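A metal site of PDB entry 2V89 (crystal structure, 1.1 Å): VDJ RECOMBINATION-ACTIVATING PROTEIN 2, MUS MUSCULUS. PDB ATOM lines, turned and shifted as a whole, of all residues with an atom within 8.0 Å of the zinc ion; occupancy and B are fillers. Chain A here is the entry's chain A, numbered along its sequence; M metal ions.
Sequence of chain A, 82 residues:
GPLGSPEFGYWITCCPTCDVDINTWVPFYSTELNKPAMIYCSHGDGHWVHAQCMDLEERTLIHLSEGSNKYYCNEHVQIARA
ND1 of His 50 is bound to the zinc ion. SG of Cys 14 is bound to the zinc ion. The zinc ion is bound by SG of Cys 18 (2.3 Å). SG of Cys 53 is bound to the zinc ion (2.3 Å). The zinc ion has four donor atoms within binding distance.
The backbone carbonyl oxygen (O) of Tyr 10 lies within hydrogen-bond range of a ring nitrogen (NE2) of His 50 (2.8 Å). The side-chain sulfur (SG) of Cys 18 lies close to the backbone NH (N) of Val 20, 3.5 Å away. N of Cys 18 sits at hydrogen-bond distance from SG of Cys 15, 3.6 Å away.
Four residues have an atom within 4 Å of the zinc ion: Cys 14, Cys 18, His 50 and Cys 53. The nearest printed residue that does not touch the zinc ion is Val 20 (4.03 Å).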
ATOM      1  N   TYR A  10      17.292   6.150   8.325  1.00  0.00           N
ATOM      2  CA  TYR A  10      17.930   5.442   7.207  1.00  0.00           C
ATOM      3  C   TYR A  10      18.321   6.428   6.126  1.00  0.00           C
ATOM      4  O   TYR A  10      19.412   6.350   5.597  1.00  0.00           O
ATOM      5  CB  TYR A  10      17.010   4.426   6.557  1.00  0.00           C
ATOM      6  CG  TYR A  10      16.809   3.208   7.438  1.00  0.00           C
ATOM      7  CD1 TYR A  10      15.733   3.052   8.289  1.00  0.00           C
ATOM      8  CD2 TYR A  10      17.798   2.220   7.357  1.00  0.00           C
ATOM      9  CE1 TYR A  10      15.610   1.894   9.065  1.00  0.00           C
ATOM     10  CE2 TYR A  10      17.710   1.095   8.107  1.00  0.00           C
ATOM     11  CZ  TYR A  10      16.631   0.952   8.960  1.00  0.00           C
ATOM     12  OH  TYR A  10      16.566  -0.203   9.693  1.00  0.00           O
ATOM     13  N   ILE A  12      19.430   9.424   5.596  1.00  0.00           N
ATOM     14  CA  ILE A  12      20.223  10.466   6.124  1.00  0.00           C
ATOM     15  C   ILE A  12      21.526  10.544   5.324  1.00  0.00           C
ATOM     16  O   ILE A  12      21.900   9.571   4.654  1.00  0.00           O
ATOM     17  CB  ILE A  12      20.636  10.208   7.588  1.00  0.00           C
ATOM     18  CG1 ILE A  12      21.474   8.924   7.798  1.00  0.00           C
ATOM     19  CG2 ILE A  12      19.411  10.238   8.495  1.00  0.00           C
ATOM     20  CD1 ILE A  12      22.061   8.781   9.180  1.00  0.00           C
ATOM     21  N   THR A  13      22.233  11.630   5.445  1.00  0.00           N
ATOM     22  CA  THR A  13      23.636  11.740   5.006  1.00  0.00           C
ATOM     23  C   THR A  13      24.524  11.284   6.129  1.00  0.00           C
ATOM     24  O   THR A  13      24.625  12.013   7.107  1.00  0.00           O
ATOM     25  CB  THR A  13      23.974  13.180   4.590  1.00  0.00           C
ATOM     26  OG1 THR A  13      23.090  13.539   3.522  1.00  0.00           O
ATOM     27  CG2 THR A  13      25.392  13.259   4.104  1.00  0.00           C
ATOM     28  N   CYS A  14      25.131  10.110   6.043  1.00  0.00           N
ATOM     29  CA  CYS A  14      25.698   9.511   7.247  1.00  0.00           C
ATOM     30  C   CYS A  14      27.097   9.938   7.580  1.00  0.00           C
ATOM     31  O   CYS A  14      27.586   9.772   8.702  1.00  0.00           O
ATOM     32  CB  CYS A  14      25.600   7.982   7.177  1.00  0.00           C
ATOM     33  SG  CYS A  14      26.897   7.147   6.164  1.00  0.00           S
ATOM     34  N   CYS A  15      27.829  10.494   6.619  1.00  0.00           N
ATOM     35  CA  CYS A  15      29.223  10.885   6.721  1.00  0.00           C
ATOM     36  C   CYS A  15      29.533  11.827   5.542  1.00  0.00           C
ATOM     37  O   CYS A  15      28.711  11.941   4.620  1.00  0.00           O
ATOM     38  CB  CYS A  15      30.132   9.687   6.764  1.00  0.00           C
ATOM     39  SG  CYS A  15      30.244   8.772   5.213  1.00  0.00           S
ATOM     40  N   PRO A  16      30.651  12.515   5.588  1.00  0.00           N
ATOM     41  CA  PRO A  16      30.916  13.493   4.496  1.00  0.00           C
ATOM     42  C   PRO A  16      31.033  12.874   3.112  1.00  0.00           C
ATOM     43  O   PRO A  16      30.854  13.647   2.138  1.00  0.00           O
ATOM     44  CB  PRO A  16      32.233  14.128   4.896  1.00  0.00           C
ATOM     45  CG  PRO A  16      32.347  13.911   6.369  1.00  0.00           C
ATOM     46  CD  PRO A  16      31.715  12.553   6.624  1.00  0.00           C
ATOM     47  N   THR A  17      31.272  11.573   2.951  1.00  0.00           N
ATOM     48  CA  THR A  17      31.312  10.954   1.622  1.00  0.00           C
ATOM     49  C   THR A  17      30.082  10.100   1.332  1.00  0.00           C
ATOM     50  O   THR A  17      30.009   9.322   0.368  1.00  0.00           O
ATOM     51  CB  THR A  17      32.595  10.116   1.521  1.00  0.00           C
ATOM     52  OG1 THR A  17      32.728   9.162   2.570  1.00  0.00           O
ATOM     53  CG2 THR A  17      33.807  11.013   1.688  1.00  0.00           C
ATOM     54  N   CYS A  18      29.045  10.166   2.117  1.00  0.00           N
ATOM     55  CA  CYS A  18      27.853   9.292   1.999  1.00  0.00           C
ATOM     56  C   CYS A  18      27.231   9.444   0.615  1.00  0.00           C
ATOM     57  O   CYS A  18      26.974  10.594   0.265  1.00  0.00           O
ATOM     58  CB  CYS A  18      26.842   9.674   3.091  1.00  0.00           C
ATOM     59  SG  CYS A  18      25.271   8.761   2.995  1.00  0.00           S
ATOM     60  N   ASP A  19      26.988   8.353  -0.026  1.00  0.00           N
ATOM     61  CA  ASP A  19      26.427   8.229  -1.360  1.00  0.00           C
ATOM     62  C   ASP A  19      24.985   7.765  -1.386  1.00  0.00           C
ATOM     63  O   ASP A  19      24.390   7.646  -2.471  1.00  0.00           O
ATOM     64  CB  ASP A  19      27.244   7.176  -2.144  1.00  0.00           C
ATOM     65  CG  ASP A  19      27.479   7.645  -3.564  1.00  0.00           C
ATOM     66  OD1 ASP A  19      27.077   8.794  -3.834  1.00  0.00           O
ATOM     67  OD2 ASP A  19      28.061   6.869  -4.337  1.00  0.00           O
ATOM     68  N   VAL A  20      24.400   7.548  -0.216  1.00  0.00           N
ATOM     69  CA  VAL A  20      23.070   6.931  -0.194  1.00  0.00           C
ATOM     70  C   VAL A  20      21.976   7.950  -0.316  1.00  0.00           C
ATOM     71  O   VAL A  20      21.847   8.935   0.438  1.00  0.00           O
ATOM     72  CB  VAL A  20      22.970   6.141   1.114  1.00  0.00           C
ATOM     73  CG1 VAL A  20      21.573   5.564   1.292  1.00  0.00           C
ATOM     74  CG2 VAL A  20      23.952   5.003   1.090  1.00  0.00           C
ATOM     75  N   ASP A  21      21.097   7.738  -1.255  1.00  0.00           N
ATOM     76  CA  ASP A  21      19.906   8.576  -1.493  1.00  0.00           C
ATOM     77  C   ASP A  21      18.738   7.687  -1.820  1.00  0.00           C
ATOM     78  O   ASP A  21      18.930   6.781  -2.635  1.00  0.00           O
ATOM     79  CB  ASP A  21      20.267   9.532  -2.629  1.00  0.00           C
ATOM     80  CG  ASP A  21      19.219  10.506  -3.091  1.00  0.00           C
ATOM     81  OD1 ASP A  21      19.592  11.610  -3.586  1.00  0.00           O
ATOM     82  OD2 ASP A  21      18.011  10.261  -3.049  1.00  0.00           O
ATOM     83  N   PRO A  36      18.828   0.558   3.520  1.00  0.00           N
ATOM     84  CA  PRO A  36      20.248   0.228   3.608  1.00  0.00           C
ATOM     85  C   PRO A  36      20.634  -0.303   5.000  1.00  0.00           C
ATOM     86  O   PRO A  36      20.158   0.201   6.017  1.00  0.00           O
ATOM     87  CB  PRO A  36      20.899   1.582   3.389  1.00  0.00           C
ATOM     88  CG  PRO A  36      19.874   2.620   3.861  1.00  0.00           C
ATOM     89  CD  PRO A  36      18.554   1.989   3.474  1.00  0.00           C
ATOM     90  N   ALA A  37      21.512  -1.300   4.956  1.00  0.00           N
ATOM     91  CA  ALA A  37      22.072  -1.801   6.209  1.00  0.00           C
ATOM     92  C   ALA A  37      22.926  -0.740   6.878  1.00  0.00           C
ATOM     93  O   ALA A  37      23.665   0.017   6.199  1.00  0.00           O
ATOM     94  CB  ALA A  37      22.903  -3.039   5.912  1.00  0.00           C
ATOM     95  N   MET A  38      22.850  -0.704   8.219  1.00  0.00           N
ATOM     96  CA  MET A  38      23.554   0.314   8.988  1.00  0.00           C
ATOM     97  C   MET A  38      24.227  -0.310  10.212  1.00  0.00           C
ATOM     98  O   MET A  38      23.816  -1.389  10.662  1.00  0.00           O
ATOM     99  CB  MET A  38      22.623   1.453   9.422  1.00  0.00           C
ATOM    100  CG  MET A  38      21.932   2.123   8.248  1.00  0.00           C
ATOM    101  SD  MET A  38      20.958   3.571   8.669  1.00  0.00           S
ATOM    102  CE  MET A  38      22.230   4.790   8.838  1.00  0.00           C
ATOM    103  N   TRP A  48      24.671   6.521  13.628  1.00  0.00           N
ATOM    104  CA  TRP A  48      24.547   5.391  12.711  1.00  0.00           C
ATOM    105  C   TRP A  48      25.116   5.717  11.344  1.00  0.00           C
ATOM    106  O   TRP A  48      24.897   6.822  10.842  1.00  0.00           O
ATOM    107  CB  TRP A  48      23.081   4.945  12.539  1.00  0.00           C
ATOM    108  CG  TRP A  48      22.480   4.348  13.778  1.00  0.00           C
ATOM    109  CD1 TRP A  48      21.928   5.000  14.877  1.00  0.00           C
ATOM    110  CD2 TRP A  48      22.360   2.968  14.047  1.00  0.00           C
ATOM    111  NE1 TRP A  48      21.489   4.076  15.785  1.00  0.00           N
ATOM    112  CE2 TRP A  48      21.745   2.801  15.308  1.00  0.00           C
ATOM    113  CE3 TRP A  48      22.739   1.825  13.321  1.00  0.00           C
ATOM    114  CZ2 TRP A  48      21.483   1.535  15.861  1.00  0.00           C
ATOM    115  CZ3 TRP A  48      22.503   0.584  13.841  1.00  0.00           C
ATOM    116  CH2 TRP A  48      21.887   0.459  15.072  1.00  0.00           C
ATOM    117  N   VAL A  49      25.825   4.759  10.744  1.00  0.00           N
ATOM    118  CA  VAL A  49      26.362   4.921   9.411  1.00  0.00           C
ATOM    119  C   VAL A  49      25.888   3.775   8.536  1.00  0.00           C
ATOM    120  O   VAL A  49      25.614   2.672   8.988  1.00  0.00           O
ATOM    121  CB  VAL A  49      27.901   5.020   9.401  1.00  0.00           C
ATOM    122  CG1 VAL A  49      28.359   6.307  10.060  1.00  0.00           C
ATOM    123  CG2 VAL A  49      28.573   3.810  10.078  1.00  0.00           C
ATOM    124  N   HIS A  50      25.772   4.103   7.236  1.00  0.00           N
ATOM    125  CA  HIS A  50      25.475   3.043   6.273  1.00  0.00           C
ATOM    126  C   HIS A  50      26.699   2.142   6.153  1.00  0.00           C
ATOM    127  O   HIS A  50      27.834   2.624   5.960  1.00  0.00           O
ATOM    128  CB  HIS A  50      25.118   3.561   4.899  1.00  0.00           C
ATOM    129  CG  HIS A  50      23.947   4.526   4.916  1.00  0.00           C
ATOM    130  ND1 HIS A  50      24.163   5.832   4.576  1.00  0.00           N
ATOM    131  CD2 HIS A  50      22.655   4.350   5.253  1.00  0.00           C
ATOM    132  CE1 HIS A  50      22.957   6.437   4.699  1.00  0.00           C
ATOM    133  NE2 HIS A  50      22.028   5.576   5.091  1.00  0.00           N
ATOM    134  N   ALA A  51      26.511   0.838   6.203  1.00  0.00           N
ATOM    135  CA  ALA A  51      27.634  -0.099   6.077  1.00  0.00           C
ATOM    136  C   ALA A  51      28.392   0.063   4.760  1.00  0.00           C
ATOM    137  O   ALA A  51      29.615  -0.027   4.696  1.00  0.00           O
ATOM    138  CB  ALA A  51      27.161  -1.522   6.260  1.00  0.00           C
ATOM    139  N   GLN A  52      27.682   0.322   3.666  1.00  0.00           N
ATOM    140  CA  GLN A  52      28.315   0.441   2.402  1.00  0.00           C
ATOM    141  C   GLN A  52      29.177   1.732   2.368  1.00  0.00           C
ATOM    142  O   GLN A  52      30.222   1.720   1.689  1.00  0.00           O
ATOM    143  CB  GLN A  52      27.280   0.461   1.276  1.00  0.00           C
ATOM    144  CG  GLN A  52      27.776   0.273  -0.085  1.00  0.00           C
ATOM    145  CD  GLN A  52      26.625  -0.118  -1.019  1.00  0.00           C
ATOM    146  OE1 GLN A  52      25.397  -0.109  -0.801  1.00  0.00           O
ATOM    147  NE2 GLN A  52      27.121  -0.518  -2.151  1.00  0.00           N
ATOM    148  N   CYS A  53      28.796   2.777   3.073  1.00  0.00           N
ATOM    149  CA  CYS A  53      29.552   4.012   3.138  1.00  0.00           C
ATOM    150  C   CYS A  53      30.859   3.814   3.888  1.00  0.00           C
ATOM    151  O   CYS A  53      31.822   4.547   3.657  1.00  0.00           O
ATOM    152  CB  CYS A  53      28.704   5.129   3.752  1.00  0.00           C
ATOM    153  SG  CYS A  53      27.273   5.543   2.728  1.00  0.00           S
ATOM    154  N   MET A  54      30.905   2.801   4.759  1.00  0.00           N
ATOM    155  CA  MET A  54      32.139   2.434   5.461  1.00  0.00           C
ATOM    156  C   MET A  54      32.971   1.424   4.696  1.00  0.00           C
ATOM    157  O   MET A  54      34.002   0.952   5.222  1.00  0.00           O
ATOM    158  CB  MET A  54      31.797   1.869   6.848  1.00  0.00           C
ATOM    159  CG  MET A  54      31.060   2.825   7.739  1.00  0.00           C
ATOM    160  SD  MET A  54      31.880   4.380   8.079  1.00  0.00           S
ATOM    161  CE  MET A  54      30.975   5.527   7.019  1.00  0.00           C
HETATM  162 ZN    ZN M   1      25.913   6.831   4.101  1.00  0.00          ZN
